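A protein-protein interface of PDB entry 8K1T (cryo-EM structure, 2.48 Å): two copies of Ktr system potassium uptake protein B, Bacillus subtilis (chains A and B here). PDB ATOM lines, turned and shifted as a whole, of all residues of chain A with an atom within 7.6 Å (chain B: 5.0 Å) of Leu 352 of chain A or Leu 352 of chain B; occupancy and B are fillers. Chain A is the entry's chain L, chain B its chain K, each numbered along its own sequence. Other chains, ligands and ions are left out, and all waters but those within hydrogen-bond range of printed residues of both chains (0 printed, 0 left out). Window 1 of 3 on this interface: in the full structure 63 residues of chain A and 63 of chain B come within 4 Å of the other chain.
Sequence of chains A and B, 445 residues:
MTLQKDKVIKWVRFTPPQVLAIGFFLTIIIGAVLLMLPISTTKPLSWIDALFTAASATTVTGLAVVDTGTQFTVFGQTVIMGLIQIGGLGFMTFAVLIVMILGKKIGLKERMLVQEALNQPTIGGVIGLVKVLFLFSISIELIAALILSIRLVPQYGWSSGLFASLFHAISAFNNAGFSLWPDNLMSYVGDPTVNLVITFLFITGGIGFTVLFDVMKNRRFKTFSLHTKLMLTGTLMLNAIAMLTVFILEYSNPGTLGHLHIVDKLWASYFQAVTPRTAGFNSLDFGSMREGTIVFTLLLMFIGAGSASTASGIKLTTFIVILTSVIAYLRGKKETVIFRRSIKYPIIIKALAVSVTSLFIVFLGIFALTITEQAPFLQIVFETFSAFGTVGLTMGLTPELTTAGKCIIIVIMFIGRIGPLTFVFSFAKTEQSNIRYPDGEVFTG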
ATOM      1  N   THR A 318      21.841  30.181 -33.900  1.00  0.00           N
ATOM      2  CA  THR A 318      21.998  29.574 -32.582  1.00  0.00           C
ATOM      3  C   THR A 318      21.683  30.574 -31.480  1.00  0.00           C
ATOM      4  O   THR A 318      21.011  30.241 -30.500  1.00  0.00           O
ATOM      5  CB  THR A 318      23.417  29.033 -32.418  1.00  0.00           C
ATOM      6  OG1 THR A 318      23.664  28.028 -33.406  1.00  0.00           O
ATOM      7  CG2 THR A 318      23.604  28.431 -31.038  1.00  0.00           C
ATOM      8  N   VAL A 321      17.820  31.212 -31.531  1.00  0.00           N
ATOM      9  CA  VAL A 321      17.039  30.069 -31.065  1.00  0.00           C
ATOM     10  C   VAL A 321      17.070  29.978 -29.545  1.00  0.00           C
ATOM     11  O   VAL A 321      16.042  29.732 -28.904  1.00  0.00           O
ATOM     12  CB  VAL A 321      17.550  28.776 -31.727  1.00  0.00           C
ATOM     13  CG1 VAL A 321      17.136  27.563 -30.927  1.00  0.00           C
ATOM     14  CG2 VAL A 321      17.020  28.672 -33.143  1.00  0.00           C
ATOM     15  N   ILE A 322      18.243  30.175 -28.945  1.00  0.00           N
ATOM     16  CA  ILE A 322      18.347  30.140 -27.490  1.00  0.00           C
ATOM     17  C   ILE A 322      17.639  31.338 -26.872  1.00  0.00           C
ATOM     18  O   ILE A 322      16.900  31.203 -25.892  1.00  0.00           O
ATOM     19  CB  ILE A 322      19.823  30.077 -27.065  1.00  0.00           C
ATOM     20  CG1 ILE A 322      20.410  28.714 -27.412  1.00  0.00           C
ATOM     21  CG2 ILE A 322      19.970  30.363 -25.580  1.00  0.00           C
ATOM     22  CD1 ILE A 322      21.879  28.620 -27.150  1.00  0.00           C
ATOM     23  N   LEU A 323      17.857  32.529 -27.432  1.00  0.00           N
ATOM     24  CA  LEU A 323      17.259  33.733 -26.867  1.00  0.00           C
ATOM     25  C   LEU A 323      15.740  33.682 -26.932  1.00  0.00           C
ATOM     26  O   LEU A 323      15.057  34.048 -25.971  1.00  0.00           O
ATOM     27  CB  LEU A 323      17.787  34.966 -27.596  1.00  0.00           C
ATOM     28  CG  LEU A 323      17.519  36.308 -26.920  1.00  0.00           C
ATOM     29  CD1 LEU A 323      18.246  36.372 -25.590  1.00  0.00           C
ATOM     30  CD2 LEU A 323      17.939  37.455 -27.823  1.00  0.00           C
ATOM     31  N   SER A 325      13.925  30.919 -27.114  1.00  0.00           N
ATOM     32  CA  SER A 325      13.482  29.852 -26.225  1.00  0.00           C
ATOM     33  C   SER A 325      13.421  30.320 -24.775  1.00  0.00           C
ATOM     34  O   SER A 325      12.508  29.942 -24.035  1.00  0.00           O
ATOM     35  CB  SER A 325      14.409  28.647 -26.359  1.00  0.00           C
ATOM     36  OG  SER A 325      14.073  27.636 -25.430  1.00  0.00           O
ATOM     37  N   VAL A 326      14.390  31.131 -24.350  1.00  0.00           N
ATOM     38  CA  VAL A 326      14.380  31.657 -22.989  1.00  0.00           C
ATOM     39  C   VAL A 326      13.242  32.649 -22.805  1.00  0.00           C
ATOM     40  O   VAL A 326      12.523  32.608 -21.801  1.00  0.00           O
ATOM     41  CB  VAL A 326      15.744  32.289 -22.655  1.00  0.00           C
ATOM     42  CG1 VAL A 326      15.664  33.082 -21.367  1.00  0.00           C
ATOM     43  CG2 VAL A 326      16.799  31.214 -22.542  1.00  0.00           C
ATOM     44  N   ILE A 327      13.058  33.554 -23.769  1.00  0.00           N
ATOM     45  CA  ILE A 327      11.993  34.548 -23.668  1.00  0.00           C
ATOM     46  C   ILE A 327      10.629  33.871 -23.650  1.00  0.00           C
ATOM     47  O   ILE A 327       9.716  34.298 -22.935  1.00  0.00           O
ATOM     48  CB  ILE A 327      12.111  35.569 -24.813  1.00  0.00           C
ATOM     49  CG1 ILE A 327      13.362  36.425 -24.629  1.00  0.00           C
ATOM     50  CG2 ILE A 327      10.879  36.449 -24.885  1.00  0.00           C
ATOM     51  CD1 ILE A 327      13.564  37.448 -25.715  1.00  0.00           C
ATOM     52  N   TYR A 329       9.992  30.903 -22.391  1.00  0.00           N
ATOM     53  CA  TYR A 329       9.826  30.353 -21.052  1.00  0.00           C
ATOM     54  C   TYR A 329       9.455  31.428 -20.038  1.00  0.00           C
ATOM     55  O   TYR A 329       8.597  31.198 -19.180  1.00  0.00           O
ATOM     56  CB  TYR A 329      11.100  29.635 -20.613  1.00  0.00           C
ATOM     57  CG  TYR A 329      11.002  29.030 -19.235  1.00  0.00           C
ATOM     58  CD1 TYR A 329      10.460  27.768 -19.052  1.00  0.00           C
ATOM     59  CD2 TYR A 329      11.440  29.724 -18.117  1.00  0.00           C
ATOM     60  CE1 TYR A 329      10.360  27.214 -17.798  1.00  0.00           C
ATOM     61  CE2 TYR A 329      11.343  29.177 -16.859  1.00  0.00           C
ATOM     62  CZ  TYR A 329      10.803  27.921 -16.704  1.00  0.00           C
ATOM     63  OH  TYR A 329      10.705  27.369 -15.450  1.00  0.00           O
ATOM     64  N   PRO A 346      14.829  19.066 -30.541  1.00  0.00           N
ATOM     65  CA  PRO A 346      16.167  18.770 -31.082  1.00  0.00           C
ATOM     66  C   PRO A 346      16.929  19.997 -31.546  1.00  0.00           C
ATOM     67  O   PRO A 346      18.163  20.010 -31.471  1.00  0.00           O
ATOM     68  CB  PRO A 346      15.865  17.822 -32.248  1.00  0.00           C
ATOM     69  CG  PRO A 346      14.630  17.143 -31.846  1.00  0.00           C
ATOM     70  CD  PRO A 346      13.814  18.171 -31.124  1.00  0.00           C
ATOM     71  N   ILE A 347      16.239  21.025 -32.038  1.00  0.00           N
ATOM     72  CA  ILE A 347      16.925  22.257 -32.410  1.00  0.00           C
ATOM     73  C   ILE A 347      17.415  22.991 -31.169  1.00  0.00           C
ATOM     74  O   ILE A 347      18.517  23.550 -31.156  1.00  0.00           O
ATOM     75  CB  ILE A 347      16.001  23.144 -33.263  1.00  0.00           C
ATOM     76  CG1 ILE A 347      15.480  22.366 -34.471  1.00  0.00           C
ATOM     77  CG2 ILE A 347      16.728  24.396 -33.707  1.00  0.00           C
ATOM     78  CD1 ILE A 347      16.568  21.839 -35.366  1.00  0.00           C
ATOM     79  N   ILE A 348      16.605  23.007 -30.110  1.00  0.00           N
ATOM     80  CA  ILE A 348      16.969  23.729 -28.895  1.00  0.00           C
ATOM     81  C   ILE A 348      18.192  23.097 -28.242  1.00  0.00           C
ATOM     82  O   ILE A 348      19.114  23.796 -27.810  1.00  0.00           O
ATOM     83  CB  ILE A 348      15.778  23.776 -27.921  1.00  0.00           C
ATOM     84  CG1 ILE A 348      14.532  24.326 -28.616  1.00  0.00           C
ATOM     85  CG2 ILE A 348      16.121  24.608 -26.699  1.00  0.00           C
ATOM     86  CD1 ILE A 348      14.649  25.763 -29.023  1.00  0.00           C
ATOM     87  N   ILE A 349      18.211  21.767 -28.144  1.00  0.00           N
ATOM     88  CA  ILE A 349      19.300  21.101 -27.440  1.00  0.00           C
ATOM     89  C   ILE A 349      20.604  21.217 -28.223  1.00  0.00           C
ATOM     90  O   ILE A 349      21.685  21.336 -27.634  1.00  0.00           O
ATOM     91  CB  ILE A 349      18.937  19.636 -27.135  1.00  0.00           C
ATOM     92  CG1 ILE A 349      20.030  18.990 -26.284  1.00  0.00           C
ATOM     93  CG2 ILE A 349      18.711  18.847 -28.411  1.00  0.00           C
ATOM     94  CD1 ILE A 349      19.754  17.555 -25.925  1.00  0.00           C
ATOM     95  N   LYS A 350      20.534  21.168 -29.554  1.00  0.00           N
ATOM     96  CA  LYS A 350      21.744  21.342 -30.349  1.00  0.00           C
ATOM     97  C   LYS A 350      22.305  22.750 -30.200  1.00  0.00           C
ATOM     98  O   LYS A 350      23.521  22.927 -30.080  1.00  0.00           O
ATOM     99  CB  LYS A 350      21.470  21.031 -31.817  1.00  0.00           C
ATOM    100  CG  LYS A 350      22.695  21.197 -32.692  1.00  0.00           C
ATOM    101  CD  LYS A 350      22.408  20.851 -34.134  1.00  0.00           C
ATOM    102  CE  LYS A 350      23.635  21.073 -34.996  1.00  0.00           C
ATOM    103  NZ  LYS A 350      23.374  20.732 -36.418  1.00  0.00           N
ATOM    104  N   ALA A 351      21.437  23.762 -30.211  1.00  0.00           N
ATOM    105  CA  ALA A 351      21.896  25.126 -29.974  1.00  0.00           C
ATOM    106  C   ALA A 351      22.464  25.271 -28.570  1.00  0.00           C
ATOM    107  O   ALA A 351      23.439  25.999 -28.356  1.00  0.00           O
ATOM    108  CB  ALA A 351      20.753  26.112 -30.198  1.00  0.00           C
ATOM    109  N   LEU A 352      22.003  24.511 -27.620  1.00  0.00           N
ATOM    110  CA  LEU A 352      22.536  24.646 -26.310  1.00  0.00           C
ATOM    111  C   LEU A 352      23.841  23.962 -26.244  1.00  0.00           C
ATOM    112  O   LEU A 352      24.759  24.438 -25.624  1.00  0.00           O
ATOM    113  CB  LEU A 352      21.624  24.066 -25.253  1.00  0.00           C
ATOM    114  CG  LEU A 352      21.940  24.296 -23.778  1.00  0.00           C
ATOM    115  CD1 LEU A 352      22.967  23.309 -23.256  1.00  0.00           C
ATOM    116  CD2 LEU A 352      22.408  25.723 -23.561  1.00  0.00           C
ATOM    117  N   ALA A 353      23.954  22.847 -26.909  1.00  0.00           N
ATOM    118  CA  ALA A 353      25.251  22.179 -26.914  1.00  0.00           C
ATOM    119  C   ALA A 353      26.316  23.033 -27.591  1.00  0.00           C
ATOM    120  O   ALA A 353      27.467  23.068 -27.147  1.00  0.00           O
ATOM    121  CB  ALA A 353      25.139  20.819 -27.598  1.00  0.00           C
ATOM    122  N   VAL A 354      25.952  23.717 -28.678  1.00  0.00           N
ATOM    123  CA  VAL A 354      26.904  24.583 -29.369  1.00  0.00           C
ATOM    124  C   VAL A 354      27.343  25.722 -28.458  1.00  0.00           C
ATOM    125  O   VAL A 354      28.533  26.041 -28.360  1.00  0.00           O
ATOM    126  CB  VAL A 354      26.292  25.119 -30.676  1.00  0.00           C
ATOM    127  CG1 VAL A 354      27.175  26.196 -31.273  1.00  0.00           C
ATOM    128  CG2 VAL A 354      26.093  23.996 -31.667  1.00  0.00           C
ATOM    129  N   SER A 355      26.385  26.349 -27.775  1.00  0.00           N
ATOM    130  CA  SER A 355      26.688  27.534 -26.981  1.00  0.00           C
ATOM    131  C   SER A 355      27.495  27.189 -25.736  1.00  0.00           C
ATOM    132  O   SER A 355      28.443  27.900 -25.391  1.00  0.00           O
ATOM    133  CB  SER A 355      25.394  28.244 -26.598  1.00  0.00           C
ATOM    134  OG  SER A 355      25.661  29.429 -25.874  1.00  0.00           O
ATOM    135  N   VAL A 356      27.129  26.111 -25.041  1.00  0.00           N
ATOM    136  CA  VAL A 356      27.821  25.755 -23.807  1.00  0.00           C
ATOM    137  C   VAL A 356      29.240  25.290 -24.099  1.00  0.00           C
ATOM    138  O   VAL A 356      30.190  25.683 -23.413  1.00  0.00           O
ATOM    139  CB  VAL A 356      27.023  24.691 -23.034  1.00  0.00           C
ATOM    140  CG1 VAL A 356      27.860  24.106 -21.916  1.00  0.00           C
ATOM    141  CG2 VAL A 356      25.762  25.297 -22.471  1.00  0.00           C
ATOM    142  N   THR A 357      29.410  24.445 -25.116  1.00  0.00           N
ATOM    143  CA  THR A 357      30.742  23.965 -25.459  1.00  0.00           C
ATOM    144  C   THR A 357      31.634  25.107 -25.924  1.00  0.00           C
ATOM    145  O   THR A 357      32.826  25.142 -25.606  1.00  0.00           O
ATOM    146  CB  THR A 357      30.649  22.883 -26.532  1.00  0.00           C
ATOM    147  OG1 THR A 357      29.649  21.931 -26.160  1.00  0.00           O
ATOM    148  CG2 THR A 357      31.977  22.164 -26.678  1.00  0.00           C
ATOM    149  N   SER A 358      31.074  26.049 -26.682  1.00  0.00           N
ATOM    150  CA  SER A 358      31.849  27.199 -27.133  1.00  0.00           C
ATOM    151  C   SER A 358      32.268  28.085 -25.967  1.00  0.00           C
ATOM    152  O   SER A 358      33.405  28.567 -25.928  1.00  0.00           O
ATOM    153  CB  SER A 358      31.044  27.997 -28.155  1.00  0.00           C
ATOM    154  OG  SER A 358      29.835  28.460 -27.589  1.00  0.00           O
ATOM    155  N   LEU A 421      31.163  21.167 -31.842  1.00  0.00           N
ATOM    156  CA  LEU A 421      30.414  19.915 -31.889  1.00  0.00           C
ATOM    157  C   LEU A 421      31.113  18.885 -32.766  1.00  0.00           C
ATOM    158  O   LEU A 421      31.253  17.720 -32.377  1.00  0.00           O
ATOM    159  CB  LEU A 421      28.991  20.160 -32.390  1.00  0.00           C
ATOM    160  CG  LEU A 421      28.018  20.885 -31.461  1.00  0.00           C
ATOM    161  CD1 LEU A 421      26.603  20.404 -31.723  1.00  0.00           C
ATOM    162  CD2 LEU A 421      28.391  20.700 -30.003  1.00  0.00           C
ATOM    163  N   THR A 444      16.350  23.621  -9.805  1.00  0.00           N
ATOM    164  CA  THR A 444      17.344  24.375 -10.558  1.00  0.00           C
ATOM    165  C   THR A 444      17.047  25.871 -10.539  1.00  0.00           C
ATOM    166  O   THR A 444      17.146  26.543 -11.567  1.00  0.00           O
ATOM    167  CB  THR A 444      17.430  23.868 -11.997  1.00  0.00           C
ATOM    168  OG1 THR A 444      16.128  23.891 -12.593  1.00  0.00           O
ATOM    169  CG2 THR A 444      17.971  22.450 -12.031  1.00  0.00           C
ATOM    170  N   ILE B 322      22.679  21.336 -16.719  1.00  0.00           N
ATOM    171  CA  ILE B 322      23.061  21.784 -18.054  1.00  0.00           C
ATOM    172  C   ILE B 322      24.288  21.027 -18.544  1.00  0.00           C
ATOM    173  O   ILE B 322      24.339  20.579 -19.694  1.00  0.00           O
ATOM    174  CB  ILE B 322      23.298  23.304 -18.057  1.00  0.00           C
ATOM    175  CG1 ILE B 322      21.973  24.041 -17.891  1.00  0.00           C
ATOM    176  CG2 ILE B 322      23.999  23.737 -19.333  1.00  0.00           C
ATOM    177  CD1 ILE B 322      22.135  25.520 -17.752  1.00  0.00           C
ATOM    178  N   VAL B 326      24.393  18.562 -21.840  1.00  0.00           N
ATOM    179  CA  VAL B 326      25.270  18.773 -22.987  1.00  0.00           C
ATOM    180  C   VAL B 326      26.128  17.542 -23.240  1.00  0.00           C
ATOM    181  O   VAL B 326      26.279  17.100 -24.384  1.00  0.00           O
ATOM    182  CB  VAL B 326      26.130  20.031 -22.774  1.00  0.00           C
ATOM    183  CG1 VAL B 326      27.233  20.107 -23.810  1.00  0.00           C
ATOM    184  CG2 VAL B 326      25.265  21.269 -22.841  1.00  0.00           C
ATOM    185  N   ILE B 348      15.325  20.861 -17.771  1.00  0.00           N
ATOM    186  CA  ILE B 348      16.393  21.357 -18.633  1.00  0.00           C
ATOM    187  C   ILE B 348      16.120  22.796 -19.052  1.00  0.00           C
ATOM    188  O   ILE B 348      17.017  23.644 -19.035  1.00  0.00           O
ATOM    189  CB  ILE B 348      16.561  20.441 -19.858  1.00  0.00           C
ATOM    190  CG1 ILE B 348      16.743  18.986 -19.426  1.00  0.00           C
ATOM    191  CG2 ILE B 348      17.736  20.898 -20.707  1.00  0.00           C
ATOM    192  CD1 ILE B 348      18.015  18.730 -18.676  1.00  0.00           C
ATOM    193  N   ILE B 349      14.882  23.090 -19.450  1.00  0.00           N
ATOM    194  CA  ILE B 349      14.574  24.420 -19.962  1.00  0.00           C
ATOM    195  C   ILE B 349      14.626  25.457 -18.845  1.00  0.00           C
ATOM    196  O   ILE B 349      15.034  26.602 -19.067  1.00  0.00           O
ATOM    197  CB  ILE B 349      13.217  24.423 -20.691  1.00  0.00           C
ATOM    198  CG1 ILE B 349      12.969  25.787 -21.334  1.00  0.00           C
ATOM    199  CG2 ILE B 349      12.085  24.058 -19.750  1.00  0.00           C
ATOM    200  CD1 ILE B 349      11.668  25.881 -22.082  1.00  0.00           C
ATOM    201  N   LYS B 350      14.202  25.087 -17.635  1.00  0.00           N
ATOM    202  CA  LYS B 350      14.296  26.020 -16.519  1.00  0.00           C
ATOM    203  C   LYS B 350      15.748  26.323 -16.172  1.00  0.00           C
ATOM    204  O   LYS B 350      16.097  27.477 -15.905  1.00  0.00           O
ATOM    205  CB  LYS B 350      13.560  25.474 -15.300  1.00  0.00           C
ATOM    206  CG  LYS B 350      13.626  26.403 -14.106  1.00  0.00           C
ATOM    207  CD  LYS B 350      12.862  25.857 -12.924  1.00  0.00           C
ATOM    208  CE  LYS B 350      12.985  26.782 -11.729  1.00  0.00           C
ATOM    209  NZ  LYS B 350      12.234  26.264 -10.556  1.00  0.00           N
ATOM    210  N   ALA B 351      16.604  25.301 -16.163  1.00  0.00           N
ATOM    211  CA  ALA B 351      18.026  25.535 -15.937  1.00  0.00           C
ATOM    212  C   ALA B 351      18.620  26.379 -17.054  1.00  0.00           C
ATOM    213  O   ALA B 351      19.492  27.221 -16.814  1.00  0.00           O
ATOM    214  CB  ALA B 351      18.764  24.206 -15.813  1.00  0.00           C
ATOM    215  N   LEU B 352      18.150  26.296 -18.265  1.00  0.00           N
ATOM    216  CA  LEU B 352      18.704  27.096 -19.303  1.00  0.00           C
ATOM    217  C   LEU B 352      18.183  28.475 -19.184  1.00  0.00           C
ATOM    218  O   LEU B 352      18.897  29.406 -19.457  1.00  0.00           O
ATOM    219  CB  LEU B 352      18.344  26.515 -20.668  1.00  0.00           C
ATOM    220  CG  LEU B 352      18.795  27.147 -21.979  1.00  0.00           C
ATOM    221  CD1 LEU B 352      18.005  28.392 -22.328  1.00  0.00           C
ATOM    222  CD2 LEU B 352      20.279  27.449 -21.917  1.00  0.00           C
ATOM    223  N   ALA B 353      16.951  28.651 -18.760  1.00  0.00           N
ATOM    224  CA  ALA B 353      16.470  30.012 -18.554  1.00  0.00           C
ATOM    225  C   ALA B 353      17.226  30.705 -17.428  1.00  0.00           C
ATOM    226  O   ALA B 353      17.523  31.901 -17.516  1.00  0.00           O
ATOM    227  CB  ALA B 353      14.970  30.001 -18.267  1.00  0.00           C
ATOM    228  N   VAL B 354      17.534  29.974 -16.355  1.00  0.00           N
ATOM    229  CA  VAL B 354      18.285  30.554 -15.245  1.00  0.00           C
ATOM    230  C   VAL B 354      19.675  30.971 -15.704  1.00  0.00           C
ATOM    231  O   VAL B 354      20.151  32.067 -15.392  1.00  0.00           O
ATOM    232  CB  VAL B 354      18.359  29.564 -14.070  1.00  0.00           C
ATOM    233  CG1 VAL B 354      19.328  30.061 -13.016  1.00  0.00           C
ATOM    234  CG2 VAL B 354      16.991  29.354 -13.465  1.00  0.00           C
ATOM    235  N   SER B 355      20.345  30.099 -16.459  1.00  0.00           N
ATOM    236  CA  SER B 355      21.730  30.351 -16.836  1.00  0.00           C
ATOM    237  C   SER B 355      21.845  31.478 -17.854  1.00  0.00           C
ATOM    238  O   SER B 355      22.734  32.328 -17.747  1.00  0.00           O
ATOM    239  CB  SER B 355      22.357  29.072 -17.382  1.00  0.00           C
ATOM    240  OG  SER B 355      23.720  29.272 -17.705  1.00  0.00           O
ATOM    241  N   VAL B 356      20.965  31.496 -18.856  1.00  0.00           N
ATOM    242  CA  VAL B 356      21.050  32.514 -19.899  1.00  0.00           C
ATOM    243  C   VAL B 356      20.699  33.886 -19.343  1.00  0.00           C
ATOM    244  O   VAL B 356      21.379  34.878 -19.629  1.00  0.00           O
ATOM    245  CB  VAL B 356      20.152  32.135 -21.089  1.00  0.00           C
ATOM    246  CG1 VAL B 356      20.006  33.307 -22.037  1.00  0.00           C
ATOM    247  CG2 VAL B 356      20.733  30.951 -21.819  1.00  0.00           C
ATOM    248  N   THR B 357      19.633  33.968 -18.547  1.00  0.00           N
ATOM    249  CA  THR B 357      19.243  35.250 -17.971  1.00  0.00           C
ATOM    250  C   THR B 357      20.312  35.774 -17.024  1.00  0.00           C
ATOM    251  O   THR B 357      20.577  36.979 -16.983  1.00  0.00           O
ATOM    252  CB  THR B 357      17.903  35.114 -17.251  1.00  0.00           C
ATOM    253  OG1 THR B 357      16.976  34.429 -18.099  1.00  0.00           O
ATOM    254  CG2 THR B 357      17.338  36.482 -16.919  1.00  0.00           C
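Leu 352 of chain A touches just these residues of chain B: Val 326 and Leu 352.
Of chain A, only Val 326 and Leu 352 come within 4 Å of Leu 352 of chain B.
Of the printed residues of chain A, Val 326 of chain B touches Leu 352 (3.1 Å), Val 356 (3.9 Å) and Thr 357 (3.8 Å).
Printed residues of chain B within 4 Å of Tyr 329 of chain A: Ile 349 (3.8 Å), Lys 350 (3.4 Å) and Ala 353 (3.5 Å).
The nearest residue of chain B that does not touch Leu 352 of chain A is Ile 322 of chain B (4.1 Å).
The nearest residue of chain A that does not touch Leu 352 of chain B is Ile 322 of chain A (4.3 Å).
The nearest printed residue of chain A that does not touch Lys 350 of chain B is Val 326 of chain A (7.6 Å).
Among the printed residues, merely in contact across the chains: Val 326 of chain A with Leu 352 of chain B (3.1 Å), Leu 352 of chain A with Val 326 of chain B (3.1 Å), Leu 352 of chain A with Leu 352 of chain B (3.2 Å), Tyr 329 of chain A with Lys 350 of chain B (3.4 Å), Thr 444 of chain A with Val 354 of chain B (3.4 Å), Tyr 329 of chain A with Ala 353 of chain B (3.5 Å), Tyr 329 of chain A with Ile 349 of chain B (3.8 Å), Val 326 of chain A with Val 356 of chain B (3.8 Å), Val 326 of chain A with Thr 357 of chain B (3.8 Å), Thr 444 of chain A with Lys 350 of chain B (3.8 Å), Thr 357 of chain A with Val 326 of chain B (3.8 Å), Val 356 of chain A with Val 326 of chain B (3.9 Å), Thr 444 of chain A with Ala 351 of chain B (3.9 Å), Ile 322 of chain A with Val 356 of chain B (3.9 Å) and Val 356 of chain A with Ile 322 of chain B (3.9 Å).
O of Ala 353 of chain B is in hydrogen-bond range of OG1 of Thr 357 of chain B (2.7 Å).
OG1 of Thr 357 of chain A lies within hydrogen-bond range of O of Ala 353 of chain A (2.7 Å).
Ile 322 of chain A touches Val 356 of chain B, and with the chains exchanged Val 356 of chain A touches Ile 322 of chain B.
Val 326 of chain A touches Leu 352 of chain B, and with the chains exchanged Leu 352 of chain A touches Val 326 of chain B.
Val 326 of chain A touches Val 356 of chain B, and with the chains exchanged Val 356 of chain A touches Val 326 of chain B.
Leu 352 of chain B touches its own counterpart, Leu 352 of chain A.
Positions printed for both chains: 322, 326, 348, 349, 350, 351, 352, 353, 354, 355, 356 and 357.
Of the 15 pairs that touch across the chains among the printed residues, 9 have their exchanged pair printed and touching as well.
Of the 23 printed residues of chain A, 7 touch a printed residue of chain B.
Printed residues of chain B that touch a printed residue of chain A: Ile 322, Val 326, Ile 349, Lys 350, Ala 351, Leu 352, Ala 353, Val 354, Val 356 and Thr 357.
Hydrophobic or aromatic side chains of chain B that line the printed part of chain A: Ile 322, Val 326, Ile 349, Leu 352, Ala 353, Val 354 and Val 356.
Along chain B the printed residues that touch a printed residue of chain A span positions 322 to 357.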
